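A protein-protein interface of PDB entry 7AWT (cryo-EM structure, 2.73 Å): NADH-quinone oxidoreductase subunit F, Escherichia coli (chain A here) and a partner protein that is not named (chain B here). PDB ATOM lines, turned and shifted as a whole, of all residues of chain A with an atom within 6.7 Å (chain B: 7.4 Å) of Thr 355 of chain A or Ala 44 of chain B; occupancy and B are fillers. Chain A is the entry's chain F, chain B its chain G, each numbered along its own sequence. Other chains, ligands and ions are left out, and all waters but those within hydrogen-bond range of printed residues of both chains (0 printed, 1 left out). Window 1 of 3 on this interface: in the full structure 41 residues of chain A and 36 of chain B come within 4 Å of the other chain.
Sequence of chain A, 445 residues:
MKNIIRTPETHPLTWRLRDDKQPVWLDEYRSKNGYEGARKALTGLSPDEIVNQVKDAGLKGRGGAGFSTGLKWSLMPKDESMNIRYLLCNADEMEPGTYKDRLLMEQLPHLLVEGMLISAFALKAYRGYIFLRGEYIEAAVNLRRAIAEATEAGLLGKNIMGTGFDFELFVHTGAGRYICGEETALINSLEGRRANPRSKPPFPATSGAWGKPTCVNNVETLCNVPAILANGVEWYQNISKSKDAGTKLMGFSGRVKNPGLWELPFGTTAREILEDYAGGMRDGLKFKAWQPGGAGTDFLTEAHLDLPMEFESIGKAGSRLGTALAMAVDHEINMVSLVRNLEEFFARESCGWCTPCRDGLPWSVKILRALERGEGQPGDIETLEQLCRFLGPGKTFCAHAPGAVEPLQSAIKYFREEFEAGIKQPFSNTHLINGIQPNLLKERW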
ATOM      1  N   GLY A 352      22.947   2.555  -3.875  1.00  0.00           N
ATOM      2  CA  GLY A 352      22.498   1.361  -3.213  1.00  0.00           C
ATOM      3  C   GLY A 352      21.367   1.491  -2.248  1.00  0.00           C
ATOM      4  O   GLY A 352      21.006   0.534  -1.609  1.00  0.00           O
ATOM      5  N   TRP A 353      20.768   2.651  -2.148  1.00  0.00           N
ATOM      6  CA  TRP A 353      19.774   2.820  -1.117  1.00  0.00           C
ATOM      7  C   TRP A 353      18.495   1.994  -1.090  1.00  0.00           C
ATOM      8  O   TRP A 353      18.214   1.369  -0.089  1.00  0.00           O
ATOM      9  CB  TRP A 353      19.435   4.296  -1.034  1.00  0.00           C
ATOM     10  CG  TRP A 353      18.748   4.685   0.170  1.00  0.00           C
ATOM     11  CD1 TRP A 353      17.443   4.879   0.304  1.00  0.00           C
ATOM     12  CD2 TRP A 353      19.325   4.952   1.438  1.00  0.00           C
ATOM     13  NE1 TRP A 353      17.149   5.248   1.569  1.00  0.00           N
ATOM     14  CE2 TRP A 353      18.299   5.296   2.290  1.00  0.00           C
ATOM     15  CE3 TRP A 353      20.616   4.925   1.930  1.00  0.00           C
ATOM     16  CZ2 TRP A 353      18.510   5.615   3.598  1.00  0.00           C
ATOM     17  CZ3 TRP A 353      20.818   5.239   3.234  1.00  0.00           C
ATOM     18  CH2 TRP A 353      19.778   5.579   4.054  1.00  0.00           C
ATOM     19  N   CYS A 354      17.789   1.848  -2.196  1.00  0.00           N
ATOM     20  CA  CYS A 354      16.499   1.168  -2.136  1.00  0.00           C
ATOM     21  C   CYS A 354      16.483  -0.129  -2.870  1.00  0.00           C
ATOM     22  O   CYS A 354      17.003  -0.225  -3.950  1.00  0.00           O
ATOM     23  CB  CYS A 354      15.407   2.089  -2.648  1.00  0.00           C
ATOM     24  SG  CYS A 354      15.183   2.019  -4.414  1.00  0.00           S
ATOM     25  N   THR A 355      15.856  -1.132  -2.293  1.00  0.00           N
ATOM     26  CA  THR A 355      15.866  -2.446  -2.900  1.00  0.00           C
ATOM     27  C   THR A 355      15.230  -2.582  -4.261  1.00  0.00           C
ATOM     28  O   THR A 355      15.750  -3.250  -5.116  1.00  0.00           O
ATOM     29  CB  THR A 355      15.132  -3.443  -2.026  1.00  0.00           C
ATOM     30  OG1 THR A 355      15.886  -3.665  -0.849  1.00  0.00           O
ATOM     31  CG2 THR A 355      15.019  -4.724  -2.732  1.00  0.00           C
ATOM     32  N   PRO A 356      14.100  -1.951  -4.489  1.00  0.00           N
ATOM     33  CA  PRO A 356      13.518  -2.218  -5.796  1.00  0.00           C
ATOM     34  C   PRO A 356      14.432  -1.843  -6.926  1.00  0.00           C
ATOM     35  O   PRO A 356      14.611  -2.647  -7.796  1.00  0.00           O
ATOM     36  CB  PRO A 356      12.305  -1.323  -5.809  1.00  0.00           C
ATOM     37  CG  PRO A 356      11.936  -1.203  -4.395  1.00  0.00           C
ATOM     38  CD  PRO A 356      13.223  -1.126  -3.664  1.00  0.00           C
ATOM     39  N   CYS A 357      15.047  -0.679  -6.886  1.00  0.00           N
ATOM     40  CA  CYS A 357      15.997  -0.305  -7.929  1.00  0.00           C
ATOM     41  C   CYS A 357      17.236  -1.188  -7.880  1.00  0.00           C
ATOM     42  O   CYS A 357      17.493  -1.974  -8.804  1.00  0.00           O
ATOM     43  CB  CYS A 357      16.375   1.168  -7.780  1.00  0.00           C
ATOM     44  SG  CYS A 357      17.724   1.727  -8.830  1.00  0.00           S
ATOM     45  N   ARG A 358      17.978  -1.111  -6.772  1.00  0.00           N
ATOM     46  CA  ARG A 358      19.299  -1.727  -6.680  1.00  0.00           C
ATOM     47  C   ARG A 358      19.263  -3.215  -6.996  1.00  0.00           C
ATOM     48  O   ARG A 358      20.176  -3.737  -7.641  1.00  0.00           O
ATOM     49  CB  ARG A 358      19.884  -1.506  -5.287  1.00  0.00           C
ATOM     50  CG  ARG A 358      20.720  -2.670  -4.791  1.00  0.00           C
ATOM     51  CD  ARG A 358      21.480  -2.346  -3.523  1.00  0.00           C
ATOM     52  NE  ARG A 358      20.588  -2.039  -2.413  1.00  0.00           N
ATOM     53  CZ  ARG A 358      19.872  -2.945  -1.760  1.00  0.00           C
ATOM     54  NH1 ARG A 358      19.940  -4.222  -2.100  1.00  0.00           N
ATOM     55  NH2 ARG A 358      19.085  -2.574  -0.763  1.00  0.00           N
ATOM     56  N   ASP A 359      18.289  -3.923  -6.450  1.00  0.00           N
ATOM     57  CA  ASP A 359      18.194  -5.356  -6.661  1.00  0.00           C
ATOM     58  C   ASP A 359      17.273  -5.885  -7.734  1.00  0.00           C
ATOM     59  O   ASP A 359      17.295  -7.055  -8.007  1.00  0.00           O
ATOM     60  CB  ASP A 359      17.861  -6.030  -5.360  1.00  0.00           C
ATOM     61  CG  ASP A 359      19.074  -6.424  -4.615  1.00  0.00           C
ATOM     62  OD1 ASP A 359      19.859  -7.175  -5.196  1.00  0.00           O
ATOM     63  OD2 ASP A 359      19.277  -5.981  -3.469  1.00  0.00           O
ATOM     64  N   GLY A 360      16.487  -5.043  -8.371  1.00  0.00           N
ATOM     65  CA  GLY A 360      15.582  -5.526  -9.385  1.00  0.00           C
ATOM     66  C   GLY A 360      16.011  -5.101 -10.766  1.00  0.00           C
ATOM     67  O   GLY A 360      15.675  -5.767 -11.748  1.00  0.00           O
ATOM     68  N   LEU A 361      16.747  -3.996 -10.870  1.00  0.00           N
ATOM     69  CA  LEU A 361      17.243  -3.609 -12.181  1.00  0.00           C
ATOM     70  C   LEU A 361      18.302  -4.590 -12.682  1.00  0.00           C
ATOM     71  O   LEU A 361      18.285  -4.936 -13.869  1.00  0.00           O
ATOM     72  CB  LEU A 361      17.783  -2.180 -12.145  1.00  0.00           C
ATOM     73  CG  LEU A 361      16.704  -1.105 -12.262  1.00  0.00           C
ATOM     74  CD1 LEU A 361      17.290   0.274 -12.071  1.00  0.00           C
ATOM     75  CD2 LEU A 361      16.011  -1.201 -13.600  1.00  0.00           C
ATOM     76  N   LEU A 391       8.458  -1.175  -9.752  1.00  0.00           N
ATOM     77  CA  LEU A 391       9.466  -0.127  -9.733  1.00  0.00           C
ATOM     78  C   LEU A 391       8.892   1.235 -10.091  1.00  0.00           C
ATOM     79  O   LEU A 391       9.649   2.201 -10.198  1.00  0.00           O
ATOM     80  CB  LEU A 391      10.610  -0.470 -10.689  1.00  0.00           C
ATOM     81  CG  LEU A 391      11.851  -1.138 -10.102  1.00  0.00           C
ATOM     82  CD1 LEU A 391      11.498  -2.460  -9.461  1.00  0.00           C
ATOM     83  CD2 LEU A 391      12.893  -1.331 -11.183  1.00  0.00           C
ATOM     84  N   THR A 396       9.743   3.076  -5.117  1.00  0.00           N
ATOM     85  CA  THR A 396      11.165   3.283  -4.901  1.00  0.00           C
ATOM     86  C   THR A 396      11.422   4.609  -4.196  1.00  0.00           C
ATOM     87  O   THR A 396      10.572   5.501  -4.176  1.00  0.00           O
ATOM     88  CB  THR A 396      11.925   3.248  -6.221  1.00  0.00           C
ATOM     89  OG1 THR A 396      11.412   4.268  -7.081  1.00  0.00           O
ATOM     90  CG2 THR A 396      11.755   1.907  -6.888  1.00  0.00           C
ATOM     91  N   PHE A 397      12.594   4.747  -3.612  1.00  0.00           N
ATOM     92  CA  PHE A 397      12.962   5.944  -2.884  1.00  0.00           C
ATOM     93  C   PHE A 397      13.067   7.215  -3.708  1.00  0.00           C
ATOM     94  O   PHE A 397      12.803   8.286  -3.220  1.00  0.00           O
ATOM     95  CB  PHE A 397      14.244   5.704  -2.119  1.00  0.00           C
ATOM     96  CG  PHE A 397      14.514   6.712  -1.068  1.00  0.00           C
ATOM     97  CD1 PHE A 397      13.875   6.649   0.122  1.00  0.00           C
ATOM     98  CD2 PHE A 397      15.423   7.696  -1.270  1.00  0.00           C
ATOM     99  CE1 PHE A 397      14.117   7.564   1.102  1.00  0.00           C
ATOM    100  CE2 PHE A 397      15.677   8.621  -0.301  1.00  0.00           C
ATOM    101  CZ  PHE A 397      15.024   8.553   0.894  1.00  0.00           C
ATOM    102  N   PHE B  33      12.956  -4.192   7.421  1.00  0.00           N
ATOM    103  CA  PHE B  33      14.345  -4.466   7.709  1.00  0.00           C
ATOM    104  C   PHE B  33      15.110  -3.277   8.241  1.00  0.00           C
ATOM    105  O   PHE B  33      15.755  -3.366   9.260  1.00  0.00           O
ATOM    106  CB  PHE B  33      15.026  -5.004   6.475  1.00  0.00           C
ATOM    107  CG  PHE B  33      14.575  -6.368   6.097  1.00  0.00           C
ATOM    108  CD1 PHE B  33      14.797  -7.420   6.931  1.00  0.00           C
ATOM    109  CD2 PHE B  33      13.935  -6.590   4.917  1.00  0.00           C
ATOM    110  CE1 PHE B  33      14.383  -8.673   6.598  1.00  0.00           C
ATOM    111  CE2 PHE B  33      13.514  -7.840   4.578  1.00  0.00           C
ATOM    112  CZ  PHE B  33      13.740  -8.885   5.419  1.00  0.00           C
ATOM    113  N   CYS B  34      14.955  -2.136   7.598  1.00  0.00           N
ATOM    114  CA  CYS B  34      15.697  -0.944   7.971  1.00  0.00           C
ATOM    115  C   CYS B  34      15.152  -0.054   9.047  1.00  0.00           C
ATOM    116  O   CYS B  34      15.743   0.946   9.317  1.00  0.00           O
ATOM    117  CB  CYS B  34      15.962  -0.083   6.760  1.00  0.00           C
ATOM    118  SG  CYS B  34      14.464   0.505   5.987  1.00  0.00           S
ATOM    119  N   SER B  41      13.577   6.352  11.247  1.00  0.00           N
ATOM    120  CA  SER B  41      13.052   5.707  10.053  1.00  0.00           C
ATOM    121  C   SER B  41      13.709   6.285   8.811  1.00  0.00           C
ATOM    122  O   SER B  41      13.796   7.507   8.661  1.00  0.00           O
ATOM    123  CB  SER B  41      11.540   5.887   9.959  1.00  0.00           C
ATOM    124  OG  SER B  41      10.887   5.393  11.110  1.00  0.00           O
ATOM    125  N   VAL B  42      14.195   5.428   7.951  1.00  0.00           N
ATOM    126  CA  VAL B  42      14.719   5.829   6.660  1.00  0.00           C
ATOM    127  C   VAL B  42      13.998   4.899   5.710  1.00  0.00           C
ATOM    128  O   VAL B  42      13.763   3.744   6.014  1.00  0.00           O
ATOM    129  CB  VAL B  42      16.217   5.664   6.524  1.00  0.00           C
ATOM    130  CG1 VAL B  42      16.910   6.345   7.670  1.00  0.00           C
ATOM    131  CG2 VAL B  42      16.580   4.207   6.469  1.00  0.00           C
ATOM    132  N   GLY B  43      13.696   5.331   4.513  1.00  0.00           N
ATOM    133  CA  GLY B  43      12.893   4.494   3.656  1.00  0.00           C
ATOM    134  C   GLY B  43      13.650   3.616   2.722  1.00  0.00           C
ATOM    135  O   GLY B  43      13.147   3.287   1.680  1.00  0.00           O
ATOM    136  N   ALA B  44      14.813   3.184   3.133  1.00  0.00           N
ATOM    137  CA  ALA B  44      15.682   2.407   2.291  1.00  0.00           C
ATOM    138  C   ALA B  44      15.349   1.066   1.790  1.00  0.00           C
ATOM    139  O   ALA B  44      15.344   0.889   0.627  1.00  0.00           O
ATOM    140  CB  ALA B  44      16.991   2.253   3.012  1.00  0.00           C
ATOM    141  N   CYS B  45      14.971   0.138   2.633  1.00  0.00           N
ATOM    142  CA  CYS B  45      14.698  -1.218   2.199  1.00  0.00           C
ATOM    143  C   CYS B  45      13.474  -1.453   1.388  1.00  0.00           C
ATOM    144  O   CYS B  45      13.395  -2.465   0.747  1.00  0.00           O
ATOM    145  CB  CYS B  45      14.591  -2.113   3.364  1.00  0.00           C
ATOM    146  SG  CYS B  45      12.957  -1.939   4.000  1.00  0.00           S
ATOM    147  N   ARG B  46      12.486  -0.589   1.566  1.00  0.00           N
ATOM    148  CA  ARG B  46      11.177  -0.570   0.956  1.00  0.00           C
ATOM    149  C   ARG B  46      10.337  -1.736   1.313  1.00  0.00           C
ATOM    150  O   ARG B  46       9.425  -1.985   0.662  1.00  0.00           O
ATOM    151  CB  ARG B  46      11.235  -0.488  -0.545  1.00  0.00           C
ATOM    152  CG  ARG B  46      12.108   0.580  -1.102  1.00  0.00           C
ATOM    153  CD  ARG B  46      11.914   1.889  -0.429  1.00  0.00           C
ATOM    154  NE  ARG B  46      10.833   2.582  -1.035  1.00  0.00           N
ATOM    155  CZ  ARG B  46      10.377   3.713  -0.567  1.00  0.00           C
ATOM    156  NH1 ARG B  46      10.905   4.223   0.495  1.00  0.00           N
ATOM    157  NH2 ARG B  46       9.398   4.319  -1.144  1.00  0.00           N
ATOM    158  N   GLN B  47      10.575  -2.401   2.403  1.00  0.00           N
ATOM    159  CA  GLN B  47       9.878  -3.622   2.721  1.00  0.00           C
ATOM    160  C   GLN B  47       8.687  -3.550   3.633  1.00  0.00           C
ATOM    161  O   GLN B  47       8.141  -4.574   3.938  1.00  0.00           O
ATOM    162  CB  GLN B  47      10.868  -4.599   3.311  1.00  0.00           C
ATOM    163  CG  GLN B  47      10.749  -5.980   2.746  1.00  0.00           C
ATOM    164  CD  GLN B  47       9.757  -6.763   3.497  1.00  0.00           C
ATOM    165  OE1 GLN B  47       9.576  -6.552   4.669  1.00  0.00           O
ATOM    166  NE2 GLN B  47       9.109  -7.676   2.832  1.00  0.00           N
ATOM    167  N   MET B  65       5.327   3.371   2.184  1.00  0.00           N
ATOM    168  CA  MET B  65       6.033   2.737   3.272  1.00  0.00           C
ATOM    169  C   MET B  65       5.513   3.141   4.623  1.00  0.00           C
ATOM    170  O   MET B  65       5.455   4.300   4.949  1.00  0.00           O
ATOM    171  CB  MET B  65       7.495   3.058   3.172  1.00  0.00           C
ATOM    172  CG  MET B  65       7.974   2.872   1.767  1.00  0.00           C
ATOM    173  SD  MET B  65       7.762   1.179   1.273  1.00  0.00           S
ATOM    174  CE  MET B  65       7.167   1.301  -0.398  1.00  0.00           C
ATOM    175  N   CYS B  67       6.825   2.966   7.592  1.00  0.00           N
ATOM    176  CA  CYS B  67       7.715   3.694   8.460  1.00  0.00           C
ATOM    177  C   CYS B  67       7.937   5.130   8.103  1.00  0.00           C
ATOM    178  O   CYS B  67       8.534   5.823   8.868  1.00  0.00           O
ATOM    179  CB  CYS B  67       9.048   3.001   8.566  1.00  0.00           C
ATOM    180  SG  CYS B  67       9.992   3.149   7.067  1.00  0.00           S
ATOM    181  N   MET B  68       7.455   5.594   6.964  1.00  0.00           N
ATOM    182  CA  MET B  68       7.643   6.980   6.557  1.00  0.00           C
ATOM    183  C   MET B  68       6.351   7.779   6.488  1.00  0.00           C
ATOM    184  O   MET B  68       6.397   8.966   6.157  1.00  0.00           O
ATOM    185  CB  MET B  68       8.353   7.043   5.204  1.00  0.00           C
ATOM    186  CG  MET B  68       9.755   6.476   5.216  1.00  0.00           C
ATOM    187  SD  MET B  68      10.855   7.382   6.308  1.00  0.00           S
ATOM    188  CE  MET B  68      11.166   8.845   5.336  1.00  0.00           C
ATOM    189  N   PHE B  87       3.838  -6.910  -3.263  1.00  0.00           N
ATOM    190  CA  PHE B  87       5.043  -6.088  -3.263  1.00  0.00           C
ATOM    191  C   PHE B  87       5.953  -6.445  -2.099  1.00  0.00           C
ATOM    192  O   PHE B  87       7.175  -6.505  -2.260  1.00  0.00           O
ATOM    193  CB  PHE B  87       4.693  -4.605  -3.217  1.00  0.00           C
ATOM    194  CG  PHE B  87       5.895  -3.709  -3.241  1.00  0.00           C
ATOM    195  CD1 PHE B  87       6.515  -3.399  -4.431  1.00  0.00           C
ATOM    196  CD2 PHE B  87       6.408  -3.188  -2.074  1.00  0.00           C
ATOM    197  CE1 PHE B  87       7.618  -2.582  -4.454  1.00  0.00           C
ATOM    198  CE2 PHE B  87       7.512  -2.370  -2.096  1.00  0.00           C
ATOM    199  CZ  PHE B  87       8.118  -2.068  -3.287  1.00  0.00           C
ATOM    200  N   SER B  90       7.642  -9.689  -3.201  1.00  0.00           N
ATOM    201  CA  SER B  90       8.619  -9.486  -4.213  1.00  0.00           C
ATOM    202  C   SER B  90       9.737  -8.748  -3.606  1.00  0.00           C
ATOM    203  O   SER B  90      10.797  -8.976  -4.006  1.00  0.00           O
ATOM    204  CB  SER B  90       8.105  -8.854  -5.455  1.00  0.00           C
ATOM    205  OG  SER B  90       8.062  -7.507  -5.224  1.00  0.00           O
ATOM    206  N   VAL B  91       9.556  -7.873  -2.645  1.00  0.00           N
ATOM    207  CA  VAL B  91      10.728  -7.229  -2.052  1.00  0.00           C
ATOM    208  C   VAL B  91      11.611  -8.215  -1.397  1.00  0.00           C
ATOM    209  O   VAL B  91      12.723  -7.965  -1.344  1.00  0.00           O
ATOM    210  CB  VAL B  91      10.449  -6.098  -1.087  1.00  0.00           C
ATOM    211  CG1 VAL B  91      11.695  -5.574  -0.434  1.00  0.00           C
ATOM    212  CG2 VAL B  91       9.890  -4.965  -1.861  1.00  0.00           C
ATOM    213  N   VAL B  92      11.154  -9.229  -0.683  1.00  0.00           N
ATOM    214  CA  VAL B  92      12.113 -10.205  -0.165  1.00  0.00           C
ATOM    215  C   VAL B  92      12.664 -11.082  -1.221  1.00  0.00           C
ATOM    216  O   VAL B  92      13.691 -11.606  -1.056  1.00  0.00           O
ATOM    217  CB  VAL B  92      11.684 -11.094   0.952  1.00  0.00           C
ATOM    218  CG1 VAL B  92      11.072 -10.303   2.038  1.00  0.00           C
ATOM    219  CG2 VAL B  92      10.825 -12.194   0.467  1.00  0.00           C
ATOM    220  N   GLU B  93      11.934 -11.341  -2.266  1.00  0.00           N
ATOM    221  CA  GLU B  93      12.483 -12.136  -3.357  1.00  0.00           C
ATOM    222  C   GLU B  93      13.711 -11.462  -3.957  1.00  0.00           C
ATOM    223  O   GLU B  93      14.700 -12.131  -4.287  1.00  0.00           O
ATOM    224  CB  GLU B  93      11.415 -12.359  -4.423  1.00  0.00           C
ATOM    225  CG  GLU B  93      11.873 -13.173  -5.605  1.00  0.00           C
ATOM    226  CD  GLU B  93      10.782 -13.333  -6.636  1.00  0.00           C
ATOM    227  OE1 GLU B  93       9.691 -12.768  -6.435  1.00  0.00           O
ATOM    228  OE2 GLU B  93      11.013 -14.019  -7.651  1.00  0.00           O
ATOM    229  N   TRP B  94      13.672 -10.135  -4.091  1.00  0.00           N
ATOM    230  CA  TRP B  94      14.825  -9.407  -4.613  1.00  0.00           C
ATOM    231  C   TRP B  94      16.034  -9.562  -3.703  1.00  0.00           C
ATOM    232  O   TRP B  94      17.164  -9.705  -4.181  1.00  0.00           O
ATOM    233  CB  TRP B  94      14.479  -7.930  -4.792  1.00  0.00           C
ATOM    234  CG  TRP B  94      13.540  -7.674  -5.920  1.00  0.00           C
ATOM    235  CD1 TRP B  94      13.482  -8.344  -7.101  1.00  0.00           C
ATOM    236  CD2 TRP B  94      12.521  -6.674  -5.975  1.00  0.00           C
ATOM    237  NE1 TRP B  94      12.488  -7.827  -7.890  1.00  0.00           N
ATOM    238  CE2 TRP B  94      11.885  -6.797  -7.220  1.00  0.00           C
ATOM    239  CE3 TRP B  94      12.087  -5.685  -5.092  1.00  0.00           C
ATOM    240  CZ2 TRP B  94      10.836  -5.973  -7.604  1.00  0.00           C
ATOM    241  CZ3 TRP B  94      11.047  -4.870  -5.473  1.00  0.00           C
ATOM    242  CH2 TRP B  94      10.433  -5.017  -6.717  1.00  0.00           C
ATOM    243  N   LEU B  95      15.823  -9.528  -2.387  1.00  0.00           N
ATOM    244  CA  LEU B  95      16.923  -9.769  -1.461  1.00  0.00           C
ATOM    245  C   LEU B  95      17.434 -11.197  -1.577  1.00  0.00           C
ATOM    246  O   LEU B  95      18.644 -11.435  -1.527  1.00  0.00           O
ATOM    247  CB  LEU B  95      16.483  -9.476  -0.031  1.00  0.00           C
ATOM    248  CG  LEU B  95      15.936  -8.076   0.221  1.00  0.00           C
ATOM    249  CD1 LEU B  95      15.553  -7.924   1.673  1.00  0.00           C
ATOM    250  CD2 LEU B  95      16.965  -7.041  -0.169  1.00  0.00           C
ATOM    251  N   ILE B 152      21.970  -7.554   3.110  1.00  0.00           N
ATOM    252  CA  ILE B 152      20.821  -7.152   2.325  1.00  0.00           C
ATOM    253  C   ILE B 152      20.794  -5.645   2.162  1.00  0.00           C
ATOM    254  O   ILE B 152      19.813  -5.096   1.748  1.00  0.00           O
ATOM    255  CB  ILE B 152      19.508  -7.587   2.960  1.00  0.00           C
ATOM    256  CG1 ILE B 152      19.280  -6.843   4.241  1.00  0.00           C
ATOM    257  CG2 ILE B 152      19.535  -9.047   3.291  1.00  0.00           C
ATOM    258  CD1 ILE B 152      18.211  -7.473   5.075  1.00  0.00           C
ATOM    259  N   ALA B 153      21.867  -4.981   2.535  1.00  0.00           N
ATOM    260  CA  ALA B 153      21.983  -3.540   2.431  1.00  0.00           C
ATOM    261  C   ALA B 153      20.867  -2.757   3.063  1.00  0.00           C
ATOM    262  O   ALA B 153      20.314  -1.892   2.441  1.00  0.00           O
ATOM    263  CB  ALA B 153      22.207  -3.098   1.006  1.00  0.00           C
ATOM    264  N   CYS B 154      20.510  -3.081   4.289  1.00  0.00           N
ATOM    265  CA  CYS B 154      19.449  -2.381   4.983  1.00  0.00           C
ATOM    266  C   CYS B 154      19.888  -1.123   5.685  1.00  0.00           C
ATOM    267  O   CYS B 154      19.065  -0.424   6.224  1.00  0.00           O
ATOM    268  CB  CYS B 154      18.811  -3.302   6.004  1.00  0.00           C
ATOM    269  SG  CYS B 154      19.906  -3.810   7.340  1.00  0.00           S
ATOM    270  N   TYR B 155      21.192  -0.923   5.779  1.00  0.00           N
ATOM    271  CA  TYR B 155      21.845   0.234   6.400  1.00  0.00           C
ATOM    272  C   TYR B 155      21.724   0.355   7.900  1.00  0.00           C
ATOM    273  O   TYR B 155      22.079   1.368   8.424  1.00  0.00           O
ATOM    274  CB  TYR B 155      21.512   1.573   5.737  1.00  0.00           C
ATOM    275  CG  TYR B 155      21.963   1.670   4.319  1.00  0.00           C
ATOM    276  CD1 TYR B 155      21.274   1.045   3.325  1.00  0.00           C
ATOM    277  CD2 TYR B 155      23.071   2.381   3.980  1.00  0.00           C
ATOM    278  CE1 TYR B 155      21.689   1.108   2.026  1.00  0.00           C
ATOM    279  CE2 TYR B 155      23.480   2.452   2.681  1.00  0.00           C
ATOM    280  CZ  TYR B 155      22.775   1.813   1.718  1.00  0.00           C
ATOM    281  OH  TYR B 155      23.162   1.867   0.425  1.00  0.00           O
ATOM    282  N   ARG B 159      23.955   3.071  10.068  1.00  0.00           N
ATOM    283  CA  ARG B 159      23.192   4.092  10.778  1.00  0.00           C
ATOM    284  C   ARG B 159      23.478   4.043  12.270  1.00  0.00           C
ATOM    285  O   ARG B 159      23.895   5.042  12.860  1.00  0.00           O
ATOM    286  CB  ARG B 159      21.700   3.936  10.501  1.00  0.00           C
ATOM    287  CG  ARG B 159      21.258   4.553   9.190  1.00  0.00           C
ATOM    288  CD  ARG B 159      19.871   4.093   8.810  1.00  0.00           C
ATOM    289  NE  ARG B 159      18.892   4.436   9.833  1.00  0.00           N
ATOM    290  CZ  ARG B 159      17.906   3.635  10.212  1.00  0.00           C
ATOM    291  NH1 ARG B 159      17.770   2.442   9.659  1.00  0.00           N
ATOM    292  NH2 ARG B 159      17.059   4.025  11.150  1.00  0.00           N
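The backbone carbonyl oxygen of Gly 352 of chain A is in hydrogen-bond range of the guanidinium group of Arg 358 of chain A (2.7 Å). The backbone NH (N) of Cys 357 of chain A sits close to the side-chain sulfur (SG) of Cys 354 of chain A (3.7 Å). The guanidinium group (NH2) of Arg 358 of chain A is in hydrogen-bond range of the side-chain hydroxyl (OG1) of Thr 355 of chain A (3.4 Å). SG of Cys 34 of chain B sits close to O of Val 42 of chain B (3.3 Å). The backbone carbonyl oxygen (O) of Gly 43 of chain B lies within hydrogen-bond range of the guanidinium group (NH1) of Arg 46 of chain B. The side-chain sulfur (SG) of Cys 45 of chain B sits close to the backbone NH (N) of Gln 47 of chain B (2.9 Å).
OH of Tyr 155 of chain B lies close to O of Gly 352 of chain A, at 3.2 Å. The side-chain hydroxyl of Thr 355 of chain A lies within hydrogen-bond range of the backbone carbonyl oxygen of Cys 45 of chain B, at 3.2 Å. The backbone carbonyl oxygen (O) of Ala 153 of chain B sits at hydrogen-bond distance from the guanidinium group (NH2) of Arg 358 of chain A (3.5 Å). O of Thr 396 of chain A is in hydrogen-bond range of NH2 of Arg 46 of chain B, at 3.5 Å. The backbone carbonyl oxygen (O) of Trp 353 of chain A sits close to the backbone carbonyl oxygen (O) of Ala 44 of chain B (3.0 Å).
Among the printed residues, pairs that only touch across the chains: Cys 354 of chain A with Ala 44 of chain B, Pro 356 of chain A with Arg 46 of chain B, Thr 355 of chain A with Ala 44 of chain B, Trp 353 of chain A with Tyr 155 of chain B, Thr 355 of chain A with Leu 95 of chain B, Arg 358 of chain A with Ile 152 of chain B, Pro 356 of chain A with Trp 94 of chain B, Trp 353 of chain A with Val 42 of chain B, Phe 397 of chain A with Gly 43 of chain B, Phe 397 of chain A with Arg 46 of chain B, Asp 359 of chain A with Trp 94 of chain B, Thr 355 of chain A with Trp 94 of chain B, Leu 391 of chain A with Trp 94 of chain B and Cys 354 of chain A with Arg 46 of chain B.
Of the printed residues of chain B, Thr 355 of chain A touches Ala 44 (3.6 Å), Cys 45 (3.2 Å), Trp 94 (3.8 Å) and Leu 95 (3.6 Å). Of chain A, only Trp 353, Cys 354 and Thr 355 come within 4 Å of Ala 44 of chain B. Printed residues of chain A within 4 Å of Tyr 155 of chain B: Gly 352 and Trp 353. Of the printed residues of chain B, Asp 359 of chain A touches Trp 94 (3.8 Å). Printed residues of chain A within 4 Å of Cys 45 of chain B: Thr 355 (3.2 Å). Of the printed residues of chain A, Ala 153 of chain B touches Arg 358 (3.5 Å). Gln 47 of chain B touches none of the printed residues of chain A. Met 65 of chain B touches none of the printed residues of chain A. The nearest residue of chain B that does not touch Thr 355 of chain A is Val 91 of chain B (4.1 Å). The nearest printed residue of chain A that does not touch Trp 94 of chain B is Gly 360 of chain A (4.1 Å).
Hydrophobic or aromatic side chains of chain B that line the printed part of chain A: Val 42, Ala 44, Trp 94, Leu 95, Ala 153 and Tyr 155. Of the 13 printed residues of chain A, 10 touch a printed residue of chain B. Printed residues of chain A that touch a printed residue of chain B: Gly 352, Trp 353, Cys 354, Thr 355, Pro 356, Arg 358, Asp 359, Leu 391, Thr 396 and Phe 397. Among the printed residues, 19 pairs touch across the chains.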
